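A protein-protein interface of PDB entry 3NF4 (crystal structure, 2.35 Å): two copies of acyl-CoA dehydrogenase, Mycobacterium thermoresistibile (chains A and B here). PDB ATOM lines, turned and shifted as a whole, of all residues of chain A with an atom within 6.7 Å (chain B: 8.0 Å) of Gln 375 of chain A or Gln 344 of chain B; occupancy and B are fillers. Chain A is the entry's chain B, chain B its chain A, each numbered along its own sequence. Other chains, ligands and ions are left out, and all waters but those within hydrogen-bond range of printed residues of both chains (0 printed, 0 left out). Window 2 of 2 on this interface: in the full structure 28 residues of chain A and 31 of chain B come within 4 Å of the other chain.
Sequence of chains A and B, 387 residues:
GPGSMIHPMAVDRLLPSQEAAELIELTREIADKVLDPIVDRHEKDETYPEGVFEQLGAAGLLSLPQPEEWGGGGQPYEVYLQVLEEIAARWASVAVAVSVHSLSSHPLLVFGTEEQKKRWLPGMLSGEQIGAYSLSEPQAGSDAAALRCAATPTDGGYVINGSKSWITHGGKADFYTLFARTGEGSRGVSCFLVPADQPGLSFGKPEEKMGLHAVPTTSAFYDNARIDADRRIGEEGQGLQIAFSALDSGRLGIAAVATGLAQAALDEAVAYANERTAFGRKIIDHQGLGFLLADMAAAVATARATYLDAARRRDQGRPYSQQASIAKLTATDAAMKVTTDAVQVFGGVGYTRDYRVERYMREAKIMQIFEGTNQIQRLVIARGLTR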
ATOM      1  N   LEU A 329      14.885 -24.282   6.333  1.00  0.00           N
ATOM      2  CA  LEU A 329      16.290 -23.876   6.310  1.00  0.00           C
ATOM      3  C   LEU A 329      17.091 -24.523   7.450  1.00  0.00           C
ATOM      4  O   LEU A 329      18.079 -25.180   7.215  1.00  0.00           O
ATOM      5  CB  LEU A 329      16.385 -22.346   6.395  1.00  0.00           C
ATOM      6  CG  LEU A 329      17.793 -21.720   6.338  1.00  0.00           C
ATOM      7  CD1 LEU A 329      18.600 -22.138   5.039  1.00  0.00           C
ATOM      8  CD2 LEU A 329      17.703 -20.209   6.462  1.00  0.00           C
ATOM      9  N   LYS A 365      21.975 -34.231   1.152  1.00  0.00           N
ATOM     10  CA  LYS A 365      22.360 -33.170   0.216  1.00  0.00           C
ATOM     11  C   LYS A 365      21.186 -32.624  -0.625  1.00  0.00           C
ATOM     12  O   LYS A 365      21.070 -31.415  -0.778  1.00  0.00           O
ATOM     13  CB  LYS A 365      23.500 -33.657  -0.665  1.00  0.00           C
ATOM     14  CG  LYS A 365      23.980 -32.637  -1.682  1.00  0.00           C
ATOM     15  CD  LYS A 365      24.662 -31.460  -0.962  1.00  0.00           C
ATOM     16  CE  LYS A 365      24.085 -30.173  -1.476  1.00  0.00           C
ATOM     17  NZ  LYS A 365      24.440 -28.999  -0.599  1.00  0.00           N
ATOM     18  N   GLN A 368      18.716 -29.937   0.953  1.00  0.00           N
ATOM     19  CA  GLN A 368      19.141 -28.537   0.886  1.00  0.00           C
ATOM     20  C   GLN A 368      18.665 -27.862  -0.419  1.00  0.00           C
ATOM     21  O   GLN A 368      18.576 -26.622  -0.496  1.00  0.00           O
ATOM     22  CB  GLN A 368      20.675 -28.407   1.036  1.00  0.00           C
ATOM     23  CG  GLN A 368      21.220 -28.655   2.471  1.00  0.00           C
ATOM     24  CD  GLN A 368      22.765 -28.494   2.599  1.00  0.00           C
ATOM     25  OE1 GLN A 368      23.518 -29.146   1.896  1.00  0.00           O
ATOM     26  NE2 GLN A 368      23.214 -27.649   3.520  1.00  0.00           N
ATOM     27  N   ILE A 369      18.349 -28.663  -1.433  1.00  0.00           N
ATOM     28  CA  ILE A 369      18.045 -28.151  -2.763  1.00  0.00           C
ATOM     29  C   ILE A 369      16.549 -28.070  -3.089  1.00  0.00           C
ATOM     30  O   ILE A 369      16.093 -27.079  -3.639  1.00  0.00           O
ATOM     31  CB  ILE A 369      18.821 -28.950  -3.877  1.00  0.00           C
ATOM     32  CG1 ILE A 369      20.278 -28.526  -3.903  1.00  0.00           C
ATOM     33  CG2 ILE A 369      18.204 -28.747  -5.318  1.00  0.00           C
ATOM     34  CD1 ILE A 369      21.138 -29.451  -4.743  1.00  0.00           C
ATOM     35  N   GLY A 372      12.304 -25.279  -2.845  1.00  0.00           N
ATOM     36  CA  GLY A 372      12.997 -24.009  -2.652  1.00  0.00           C
ATOM     37  C   GLY A 372      14.401 -24.153  -2.043  1.00  0.00           C
ATOM     38  O   GLY A 372      14.562 -24.494  -0.832  1.00  0.00           O
ATOM     39  N   THR A 373      15.428 -23.894  -2.857  1.00  0.00           N
ATOM     40  CA  THR A 373      16.811 -23.981  -2.359  1.00  0.00           C
ATOM     41  C   THR A 373      16.994 -23.088  -1.119  1.00  0.00           C
ATOM     42  O   THR A 373      16.303 -22.091  -0.950  1.00  0.00           O
ATOM     43  CB  THR A 373      17.874 -23.556  -3.405  1.00  0.00           C
ATOM     44  OG1 THR A 373      17.820 -22.140  -3.576  1.00  0.00           O
ATOM     45  CG2 THR A 373      17.662 -24.242  -4.786  1.00  0.00           C
ATOM     46  N   ASN A 374      17.936 -23.448  -0.265  1.00  0.00           N
ATOM     47  CA  ASN A 374      18.219 -22.655   0.932  1.00  0.00           C
ATOM     48  C   ASN A 374      18.610 -21.173   0.722  1.00  0.00           C
ATOM     49  O   ASN A 374      18.346 -20.359   1.602  1.00  0.00           O
ATOM     50  CB  ASN A 374      19.205 -23.406   1.833  1.00  0.00           C
ATOM     51  CG  ASN A 374      18.555 -24.618   2.491  1.00  0.00           C
ATOM     52  OD1 ASN A 374      17.369 -24.908   2.235  1.00  0.00           O
ATOM     53  ND2 ASN A 374      19.317 -25.334   3.344  1.00  0.00           N
ATOM     54  N   GLN A 375      19.176 -20.838  -0.449  1.00  0.00           N
ATOM     55  CA  GLN A 375      19.459 -19.438  -0.849  1.00  0.00           C
ATOM     56  C   GLN A 375      18.172 -18.678  -1.098  1.00  0.00           C
ATOM     57  O   GLN A 375      18.012 -17.522  -0.690  1.00  0.00           O
ATOM     58  CB  GLN A 375      20.344 -19.372  -2.101  1.00  0.00           C
ATOM     59  CG  GLN A 375      21.811 -19.784  -1.827  1.00  0.00           C
ATOM     60  CD  GLN A 375      21.938 -21.296  -1.554  1.00  0.00           C
ATOM     61  OE1 GLN A 375      21.372 -22.115  -2.296  1.00  0.00           O
ATOM     62  NE2 GLN A 375      22.672 -21.662  -0.475  1.00  0.00           N
ATOM     63  N   ILE A 376      17.254 -19.356  -1.766  1.00  0.00           N
ATOM     64  CA  ILE A 376      15.931 -18.833  -2.004  1.00  0.00           C
ATOM     65  C   ILE A 376      15.139 -18.695  -0.683  1.00  0.00           C
ATOM     66  O   ILE A 376      14.430 -17.692  -0.523  1.00  0.00           O
ATOM     67  CB  ILE A 376      15.238 -19.614  -3.185  1.00  0.00           C
ATOM     68  CG1 ILE A 376      15.457 -18.813  -4.477  1.00  0.00           C
ATOM     69  CG2 ILE A 376      13.763 -19.847  -2.951  1.00  0.00           C
ATOM     70  CD1 ILE A 376      15.633 -19.643  -5.709  1.00  0.00           C
ATOM     71  N   GLN A 377      15.292 -19.630   0.268  1.00  0.00           N
ATOM     72  CA  GLN A 377      14.751 -19.410   1.644  1.00  0.00           C
ATOM     73  C   GLN A 377      15.326 -18.137   2.334  1.00  0.00           C
ATOM     74  O   GLN A 377      14.578 -17.378   2.928  1.00  0.00           O
ATOM     75  CB  GLN A 377      14.941 -20.609   2.605  1.00  0.00           C
ATOM     76  CG  GLN A 377      14.379 -21.975   2.187  1.00  0.00           C
ATOM     77  CD  GLN A 377      12.910 -21.930   1.757  1.00  0.00           C
ATOM     78  OE1 GLN A 377      12.101 -21.133   2.271  1.00  0.00           O
ATOM     79  NE2 GLN A 377      12.558 -22.809   0.816  1.00  0.00           N
ATOM     80  N   ARG A 378      16.634 -17.916   2.257  1.00  0.00           N
ATOM     81  CA  ARG A 378      17.230 -16.694   2.823  1.00  0.00           C
ATOM     82  C   ARG A 378      16.663 -15.379   2.206  1.00  0.00           C
ATOM     83  O   ARG A 378      16.374 -14.395   2.916  1.00  0.00           O
ATOM     84  CB  ARG A 378      18.773 -16.734   2.746  1.00  0.00           C
ATOM     85  CG  ARG A 378      19.440 -17.811   3.645  1.00  0.00           C
ATOM     86  CD  ARG A 378      21.002 -17.860   3.521  1.00  0.00           C
ATOM     87  NE  ARG A 378      21.563 -18.757   4.539  1.00  0.00           N
ATOM     88  CZ  ARG A 378      21.795 -20.064   4.365  1.00  0.00           C
ATOM     89  NH1 ARG A 378      21.535 -20.644   3.196  1.00  0.00           N
ATOM     90  NH2 ARG A 378      22.259 -20.809   5.376  1.00  0.00           N
ATOM     91  N   LEU A 379      16.502 -15.383   0.883  1.00  0.00           N
ATOM     92  CA  LEU A 379      15.860 -14.303   0.140  1.00  0.00           C
ATOM     93  C   LEU A 379      14.439 -13.990   0.640  1.00  0.00           C
ATOM     94  O   LEU A 379      14.097 -12.845   0.882  1.00  0.00           O
ATOM     95  CB  LEU A 379      15.771 -14.727  -1.321  1.00  0.00           C
ATOM     96  CG  LEU A 379      15.747 -13.634  -2.371  1.00  0.00           C
ATOM     97  CD1 LEU A 379      17.215 -13.189  -2.589  1.00  0.00           C
ATOM     98  CD2 LEU A 379      15.068 -14.145  -3.686  1.00  0.00           C
ATOM     99  N   VAL A 380      13.631 -15.029   0.792  1.00  0.00           N
ATOM    100  CA  VAL A 380      12.270 -14.937   1.330  1.00  0.00           C
ATOM    101  C   VAL A 380      12.230 -14.329   2.744  1.00  0.00           C
ATOM    102  O   VAL A 380      11.402 -13.460   3.036  1.00  0.00           O
ATOM    103  CB  VAL A 380      11.595 -16.347   1.281  1.00  0.00           C
ATOM    104  CG1 VAL A 380      10.373 -16.451   2.199  1.00  0.00           C
ATOM    105  CG2 VAL A 380      11.250 -16.752  -0.196  1.00  0.00           C
ATOM    106  N   ALA B 269      31.963 -25.337 -10.706  1.00  0.00           N
ATOM    107  CA  ALA B 269      30.905 -24.447 -10.223  1.00  0.00           C
ATOM    108  C   ALA B 269      30.992 -23.029 -10.820  1.00  0.00           C
ATOM    109  O   ALA B 269      29.964 -22.428 -11.150  1.00  0.00           O
ATOM    110  CB  ALA B 269      30.886 -24.399  -8.681  1.00  0.00           C
ATOM    111  N   TYR B 272      29.690 -23.443 -14.493  1.00  0.00           N
ATOM    112  CA  TYR B 272      28.218 -23.521 -14.428  1.00  0.00           C
ATOM    113  C   TYR B 272      27.505 -22.208 -14.080  1.00  0.00           C
ATOM    114  O   TYR B 272      26.529 -21.847 -14.730  1.00  0.00           O
ATOM    115  CB  TYR B 272      27.745 -24.596 -13.440  1.00  0.00           C
ATOM    116  CG  TYR B 272      26.256 -24.927 -13.592  1.00  0.00           C
ATOM    117  CD1 TYR B 272      25.808 -25.731 -14.648  1.00  0.00           C
ATOM    118  CD2 TYR B 272      25.299 -24.422 -12.705  1.00  0.00           C
ATOM    119  CE1 TYR B 272      24.440 -26.049 -14.799  1.00  0.00           C
ATOM    120  CE2 TYR B 272      23.941 -24.726 -12.852  1.00  0.00           C
ATOM    121  CZ  TYR B 272      23.523 -25.536 -13.902  1.00  0.00           C
ATOM    122  OH  TYR B 272      22.190 -25.844 -14.067  1.00  0.00           O
ATOM    123  N   ILE B 283      23.079 -17.559 -13.978  1.00  0.00           N
ATOM    124  CA  ILE B 283      22.748 -18.377 -12.806  1.00  0.00           C
ATOM    125  C   ILE B 283      23.344 -17.786 -11.530  1.00  0.00           C
ATOM    126  O   ILE B 283      22.764 -17.920 -10.455  1.00  0.00           O
ATOM    127  CB  ILE B 283      23.208 -19.864 -12.976  1.00  0.00           C
ATOM    128  CG1 ILE B 283      22.482 -20.555 -14.148  1.00  0.00           C
ATOM    129  CG2 ILE B 283      23.007 -20.661 -11.682  1.00  0.00           C
ATOM    130  CD1 ILE B 283      21.114 -21.207 -13.800  1.00  0.00           C
ATOM    131  N   HIS B 286      20.587 -15.111 -10.454  1.00  0.00           N
ATOM    132  CA  HIS B 286      19.397 -15.903 -10.095  1.00  0.00           C
ATOM    133  C   HIS B 286      19.743 -17.161  -9.282  1.00  0.00           C
ATOM    134  O   HIS B 286      18.892 -17.727  -8.585  1.00  0.00           O
ATOM    135  CB  HIS B 286      18.601 -16.291 -11.354  1.00  0.00           C
ATOM    136  N   GLY B 288      21.979 -15.484  -3.872  1.00  0.00           N
ATOM    137  CA  GLY B 288      23.240 -14.993  -3.285  1.00  0.00           C
ATOM    138  C   GLY B 288      24.343 -16.012  -3.548  1.00  0.00           C
ATOM    139  O   GLY B 288      25.152 -16.379  -2.645  1.00  0.00           O
ATOM    140  N   LEU B 289      24.365 -16.466  -4.804  1.00  0.00           N
ATOM    141  CA  LEU B 289      25.355 -17.434  -5.248  1.00  0.00           C
ATOM    142  C   LEU B 289      26.765 -16.856  -5.330  1.00  0.00           C
ATOM    143  O   LEU B 289      27.735 -17.596  -5.174  1.00  0.00           O
ATOM    144  CB  LEU B 289      24.926 -18.063  -6.574  1.00  0.00           C
ATOM    145  CG  LEU B 289      24.266 -19.433  -6.428  1.00  0.00           C
ATOM    146  CD1 LEU B 289      22.841 -19.357  -5.862  1.00  0.00           C
ATOM    147  CD2 LEU B 289      24.294 -20.090  -7.801  1.00  0.00           C
ATOM    148  N   GLY B 290      26.866 -15.539  -5.543  1.00  0.00           N
ATOM    149  CA  GLY B 290      28.148 -14.827  -5.594  1.00  0.00           C
ATOM    150  C   GLY B 290      28.957 -14.966  -4.307  1.00  0.00           C
ATOM    151  O   GLY B 290      30.156 -15.270  -4.351  1.00  0.00           O
ATOM    152  N   LEU B 292      28.442 -17.330  -1.957  1.00  0.00           N
ATOM    153  CA  LEU B 292      28.799 -18.732  -1.775  1.00  0.00           C
ATOM    154  C   LEU B 292      30.085 -19.082  -2.568  1.00  0.00           C
ATOM    155  O   LEU B 292      30.989 -19.708  -2.014  1.00  0.00           O
ATOM    156  CB  LEU B 292      27.636 -19.618  -2.197  1.00  0.00           C
ATOM    157  CG  LEU B 292      27.474 -21.034  -1.681  1.00  0.00           C
ATOM    158  CD1 LEU B 292      26.882 -21.014  -0.265  1.00  0.00           C
ATOM    159  CD2 LEU B 292      26.545 -21.777  -2.607  1.00  0.00           C
ATOM    160  N   MET B 296      33.948 -20.173  -1.233  1.00  0.00           N
ATOM    161  CA  MET B 296      34.655 -21.311  -1.850  1.00  0.00           C
ATOM    162  C   MET B 296      36.084 -20.934  -2.362  1.00  0.00           C
ATOM    163  O   MET B 296      37.057 -21.687  -2.123  1.00  0.00           O
ATOM    164  CB  MET B 296      33.824 -21.953  -3.002  1.00  0.00           C
ATOM    165  CG  MET B 296      32.458 -22.581  -2.569  1.00  0.00           C
ATOM    166  SD  MET B 296      31.292 -22.940  -3.961  1.00  0.00           S
ATOM    167  CE  MET B 296      32.279 -23.954  -5.068  1.00  0.00           C
ATOM    168  N   LYS B 337      33.867 -28.811   2.644  1.00  0.00           N
ATOM    169  CA  LYS B 337      32.987 -27.629   2.490  1.00  0.00           C
ATOM    170  C   LYS B 337      32.799 -27.154   1.034  1.00  0.00           C
ATOM    171  O   LYS B 337      31.683 -26.803   0.646  1.00  0.00           O
ATOM    172  CB  LYS B 337      33.503 -26.470   3.360  1.00  0.00           C
ATOM    173  CG  LYS B 337      32.626 -25.233   3.384  1.00  0.00           C
ATOM    174  CD  LYS B 337      33.469 -23.964   3.656  1.00  0.00           C
ATOM    175  CE  LYS B 337      32.626 -22.657   3.523  1.00  0.00           C
ATOM    176  NZ  LYS B 337      33.237 -21.491   4.269  1.00  0.00           N
ATOM    177  N   VAL B 338      33.880 -27.111   0.245  1.00  0.00           N
ATOM    178  CA  VAL B 338      33.815 -26.664  -1.164  1.00  0.00           C
ATOM    179  C   VAL B 338      33.053 -27.660  -2.064  1.00  0.00           C
ATOM    180  O   VAL B 338      32.282 -27.248  -2.923  1.00  0.00           O
ATOM    181  CB  VAL B 338      35.241 -26.383  -1.730  1.00  0.00           C
ATOM    182  CG1 VAL B 338      35.242 -26.178  -3.210  1.00  0.00           C
ATOM    183  CG2 VAL B 338      35.921 -25.163  -0.980  1.00  0.00           C
ATOM    184  N   THR B 339      33.245 -28.966  -1.861  1.00  0.00           N
ATOM    185  CA  THR B 339      32.565 -29.950  -2.723  1.00  0.00           C
ATOM    186  C   THR B 339      31.056 -29.968  -2.446  1.00  0.00           C
ATOM    187  O   THR B 339      30.256 -30.123  -3.395  1.00  0.00           O
ATOM    188  CB  THR B 339      33.137 -31.370  -2.565  1.00  0.00           C
ATOM    189  OG1 THR B 339      33.202 -31.713  -1.172  1.00  0.00           O
ATOM    190  CG2 THR B 339      34.536 -31.507  -3.182  1.00  0.00           C
ATOM    191  N   THR B 340      30.681 -29.819  -1.158  1.00  0.00           N
ATOM    192  CA  THR B 340      29.292 -29.729  -0.700  1.00  0.00           C
ATOM    193  C   THR B 340      28.530 -28.486  -1.231  1.00  0.00           C
ATOM    194  O   THR B 340      27.356 -28.580  -1.614  1.00  0.00           O
ATOM    195  CB  THR B 340      29.196 -29.732   0.869  1.00  0.00           C
ATOM    196  OG1 THR B 340      29.648 -31.005   1.364  1.00  0.00           O
ATOM    197  CG2 THR B 340      27.740 -29.483   1.345  1.00  0.00           C
ATOM    198  N   ASP B 341      29.198 -27.336  -1.212  1.00  0.00           N
ATOM    199  CA  ASP B 341      28.689 -26.104  -1.833  1.00  0.00           C
ATOM    200  C   ASP B 341      28.724 -26.122  -3.392  1.00  0.00           C
ATOM    201  O   ASP B 341      27.939 -25.425  -4.028  1.00  0.00           O
ATOM    202  CB  ASP B 341      29.485 -24.890  -1.307  1.00  0.00           C
ATOM    203  CG  ASP B 341      29.184 -24.561   0.172  1.00  0.00           C
ATOM    204  OD1 ASP B 341      28.131 -24.963   0.716  1.00  0.00           O
ATOM    205  OD2 ASP B 341      30.018 -23.900   0.809  1.00  0.00           O
ATOM    206  N   ALA B 342      29.610 -26.906  -4.002  1.00  0.00           N
ATOM    207  CA  ALA B 342      29.604 -26.997  -5.450  1.00  0.00           C
ATOM    208  C   ALA B 342      28.343 -27.723  -6.010  1.00  0.00           C
ATOM    209  O   ALA B 342      27.869 -27.359  -7.096  1.00  0.00           O
ATOM    210  CB  ALA B 342      30.930 -27.579  -6.022  1.00  0.00           C
ATOM    211  N   VAL B 343      27.829 -28.735  -5.300  1.00  0.00           N
ATOM    212  CA  VAL B 343      26.578 -29.410  -5.666  1.00  0.00           C
ATOM    213  C   VAL B 343      25.454 -28.381  -5.517  1.00  0.00           C
ATOM    214  O   VAL B 343      24.559 -28.302  -6.349  1.00  0.00           O
ATOM    215  CB  VAL B 343      26.287 -30.632  -4.727  1.00  0.00           C
ATOM    216  CG1 VAL B 343      24.902 -31.291  -5.039  1.00  0.00           C
ATOM    217  CG2 VAL B 343      27.353 -31.649  -4.903  1.00  0.00           C
ATOM    218  N   GLN B 344      25.518 -27.604  -4.437  1.00  0.00           N
ATOM    219  CA  GLN B 344      24.571 -26.530  -4.167  1.00  0.00           C
ATOM    220  C   GLN B 344      24.444 -25.511  -5.342  1.00  0.00           C
ATOM    221  O   GLN B 344      23.330 -25.185  -5.765  1.00  0.00           O
ATOM    222  CB  GLN B 344      24.937 -25.841  -2.826  1.00  0.00           C
ATOM    223  CG  GLN B 344      23.811 -24.965  -2.184  1.00  0.00           C
ATOM    224  CD  GLN B 344      22.594 -25.777  -1.786  1.00  0.00           C
ATOM    225  OE1 GLN B 344      22.694 -26.994  -1.577  1.00  0.00           O
ATOM    226  NE2 GLN B 344      21.422 -25.111  -1.698  1.00  0.00           N
ATOM    227  N   VAL B 345      25.582 -25.041  -5.867  1.00  0.00           N
ATOM    228  CA  VAL B 345      25.633 -24.145  -7.049  1.00  0.00           C
ATOM    229  C   VAL B 345      24.907 -24.722  -8.313  1.00  0.00           C
ATOM    230  O   VAL B 345      24.177 -24.000  -8.997  1.00  0.00           O
ATOM    231  CB  VAL B 345      27.098 -23.707  -7.350  1.00  0.00           C
ATOM    232  CG1 VAL B 345      27.206 -22.983  -8.670  1.00  0.00           C
ATOM    233  CG2 VAL B 345      27.660 -22.832  -6.189  1.00  0.00           C
ATOM    234  N   PHE B 346      25.063 -26.021  -8.584  1.00  0.00           N
ATOM    235  CA  PHE B 346      24.368 -26.647  -9.724  1.00  0.00           C
ATOM    236  C   PHE B 346      22.822 -26.806  -9.577  1.00  0.00           C
ATOM    237  O   PHE B 346      22.111 -26.940 -10.581  1.00  0.00           O
ATOM    238  CB  PHE B 346      25.002 -27.999 -10.064  1.00  0.00           C
ATOM    239  CG  PHE B 346      26.294 -27.908 -10.863  1.00  0.00           C
ATOM    240  CD1 PHE B 346      27.480 -27.454 -10.264  1.00  0.00           C
ATOM    241  CD2 PHE B 346      26.334 -28.325 -12.194  1.00  0.00           C
ATOM    242  CE1 PHE B 346      28.678 -27.407 -10.968  1.00  0.00           C
ATOM    243  CE2 PHE B 346      27.543 -28.263 -12.954  1.00  0.00           C
ATOM    244  CZ  PHE B 346      28.720 -27.809 -12.328  1.00  0.00           C
ATOM    245  N   GLY B 347      22.300 -26.796  -8.343  1.00  0.00           N
ATOM    246  CA  GLY B 347      20.889 -27.100  -8.117  1.00  0.00           C
ATOM    247  C   GLY B 347      20.609 -28.579  -8.362  1.00  0.00           C
ATOM    248  O   GLY B 347      21.497 -29.424  -8.192  1.00  0.00           O
ATOM    249  N   GLY B 348      19.373 -28.897  -8.777  1.00  0.00           N
ATOM    250  CA  GLY B 348      18.934 -30.284  -8.957  1.00  0.00           C
ATOM    251  C   GLY B 348      19.810 -31.126  -9.873  1.00  0.00           C
ATOM    252  O   GLY B 348      20.043 -32.315  -9.578  1.00  0.00           O
ATOM    253  N   GLY B 350      22.934 -30.902 -10.239  1.00  0.00           N
ATOM    254  CA  GLY B 350      24.130 -31.189  -9.441  1.00  0.00           C
ATOM    255  C   GLY B 350      24.057 -32.507  -8.675  1.00  0.00           C
ATOM    256  O   GLY B 350      25.075 -33.167  -8.459  1.00  0.00           O
ATOM    257  N   TYR B 351      22.840 -32.903  -8.310  1.00  0.00           N
ATOM    258  CA  TYR B 351      22.595 -34.164  -7.635  1.00  0.00           C
ATOM    259  C   TYR B 351      22.509 -35.383  -8.577  1.00  0.00           C
ATOM    260  O   TYR B 351      22.232 -36.512  -8.122  1.00  0.00           O
ATOM    261  CB  TYR B 351      21.290 -34.030  -6.842  1.00  0.00           C
ATOM    262  CG  TYR B 351      21.049 -35.057  -5.755  1.00  0.00           C
ATOM    263  CD1 TYR B 351      21.790 -35.048  -4.588  1.00  0.00           C
ATOM    264  CD2 TYR B 351      20.034 -36.011  -5.879  1.00  0.00           C
ATOM    265  CE1 TYR B 351      21.541 -35.981  -3.569  1.00  0.00           C
ATOM    266  CE2 TYR B 351      19.778 -36.937  -4.874  1.00  0.00           C
ATOM    267  CZ  TYR B 351      20.538 -36.912  -3.725  1.00  0.00           C
ATOM    268  OH  TYR B 351      20.312 -37.815  -2.729  1.00  0.00           O
ATOM    269  N   VAL B 357      30.344 -33.214  -9.954  1.00  0.00           N
ATOM    270  CA  VAL B 357      30.350 -32.667  -8.583  1.00  0.00           C
ATOM    271  C   VAL B 357      29.808 -33.631  -7.483  1.00  0.00           C
ATOM    272  O   VAL B 357      30.264 -33.577  -6.336  1.00  0.00           O
ATOM    273  CB  VAL B 357      29.709 -31.253  -8.502  1.00  0.00           C
ATOM    274  CG1 VAL B 357      30.556 -30.268  -9.275  1.00  0.00           C
ATOM    275  CG2 VAL B 357      28.266 -31.253  -9.056  1.00  0.00           C
ATOM    276  N   MET B 361      32.134 -34.665  -4.040  1.00  0.00           N
ATOM    277  CA  MET B 361      31.585 -34.718  -2.690  1.00  0.00           C
ATOM    278  C   MET B 361      31.757 -36.059  -1.954  1.00  0.00           C
ATOM    279  O   MET B 361      32.029 -36.075  -0.765  1.00  0.00           O
ATOM    280  CB  MET B 361      30.105 -34.304  -2.692  1.00  0.00           C
ATOM    281  CG  MET B 361      29.565 -34.089  -1.309  1.00  0.00           C
ATOM    282  SD  MET B 361      27.869 -33.458  -1.286  1.00  0.00           S
ATOM    283  CE  MET B 361      27.406 -33.826   0.411  1.00  0.00           C
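OE1 of Gln 368 of chain A sits at hydrogen-bond distance from NZ of Lys 365 of chain A (2.7 Å).
The backbone carbonyl oxygen (O) of Gln 368 of chain A sits at hydrogen-bond distance from the backbone NH (N) of Asn 374 of chain A (3.2 Å).
Lys 365 of chain A touches Val 343 of chain B.
Lys 365 of chain A touches Met 361 of chain B (CD to SD, 3.8 Å).
Ile 369 of chain A touches Val 343 of chain B.
Gln 344 of chain B touches Ile 369 of chain A.
CD1 of Ile 369 of chain A touches O of Gly 347 of chain B (3.5 Å).
N of Gly 348 of chain B touches CG2 of Ile 369 of chain A (3.7 Å).
No position is printed for both chains.
Of the 25 printed residues of chain B, 6 touch a printed residue of chain A.
Printed residues of chain B that touch a printed residue of chain A: Thr 340, Val 343, Gln 344, Gly 347, Gly 348 and Met 361.
Hydrophobic or aromatic side chains of chain B within 4 Å of the printed part of chain A: Val 343 and Met 361.
Of the 13 printed residues of chain A, 4 touch a printed residue of chain B.
Printed residues of chain A that touch a printed residue of chain B: Lys 365, Gln 368, Ile 369 and Gln 375.
Hydrophobic or aromatic side chains of chain A within 4 Å of the printed part of chain B: Ile 369.
Among the printed residues, no Asp or Glu carboxylate lies within 4 Å of a Lys or Arg side-chain nitrogen of the other chain.
Of the printed residues of chain B, Gln 368 of chain A touches Gln 344 (3.4 Å).
Of chain B, only Gln 344 (3.1 Å) comes within 4 Å of Gln 375 of chain A.
Asp 341 of chain B touches none of the printed residues of chain A.
Of chain A, only Lys 365 (2.8 Å), Gln 368 (3.4 Å), Ile 369 (3.7 Å) and Gln 375 (3.1 Å) come within 4 Å of Gln 344 of chain B.
Val 345 of chain B touches none of the printed residues of chain A.
Printed residues of chain A within 4 Å of Gly 348 of chain B: Ile 369.
Printed residues of chain A within 4 Å of Met 361 of chain B: Lys 365.
The side-chain amide oxygen of Gln 344 of chain B is in hydrogen-bond range of the side-chain amino group of Lys 365 of chain A (2.8 Å).
The side-chain amide nitrogen (NE2) of Gln 344 of chain B is in hydrogen-bond range of the side-chain amide oxygen (OE1) of Gln 375 of chain A.
The side-chain amide nitrogen of Gln 344 of chain B lies within hydrogen-bond range of the backbone carbonyl oxygen of Gln 368 of chain A, at 3.4 Å.
The backbone carbonyl oxygen (O) of Thr 340 of chain B lies within hydrogen-bond range of the side-chain amino group (NZ) of Lys 365 of chain A.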
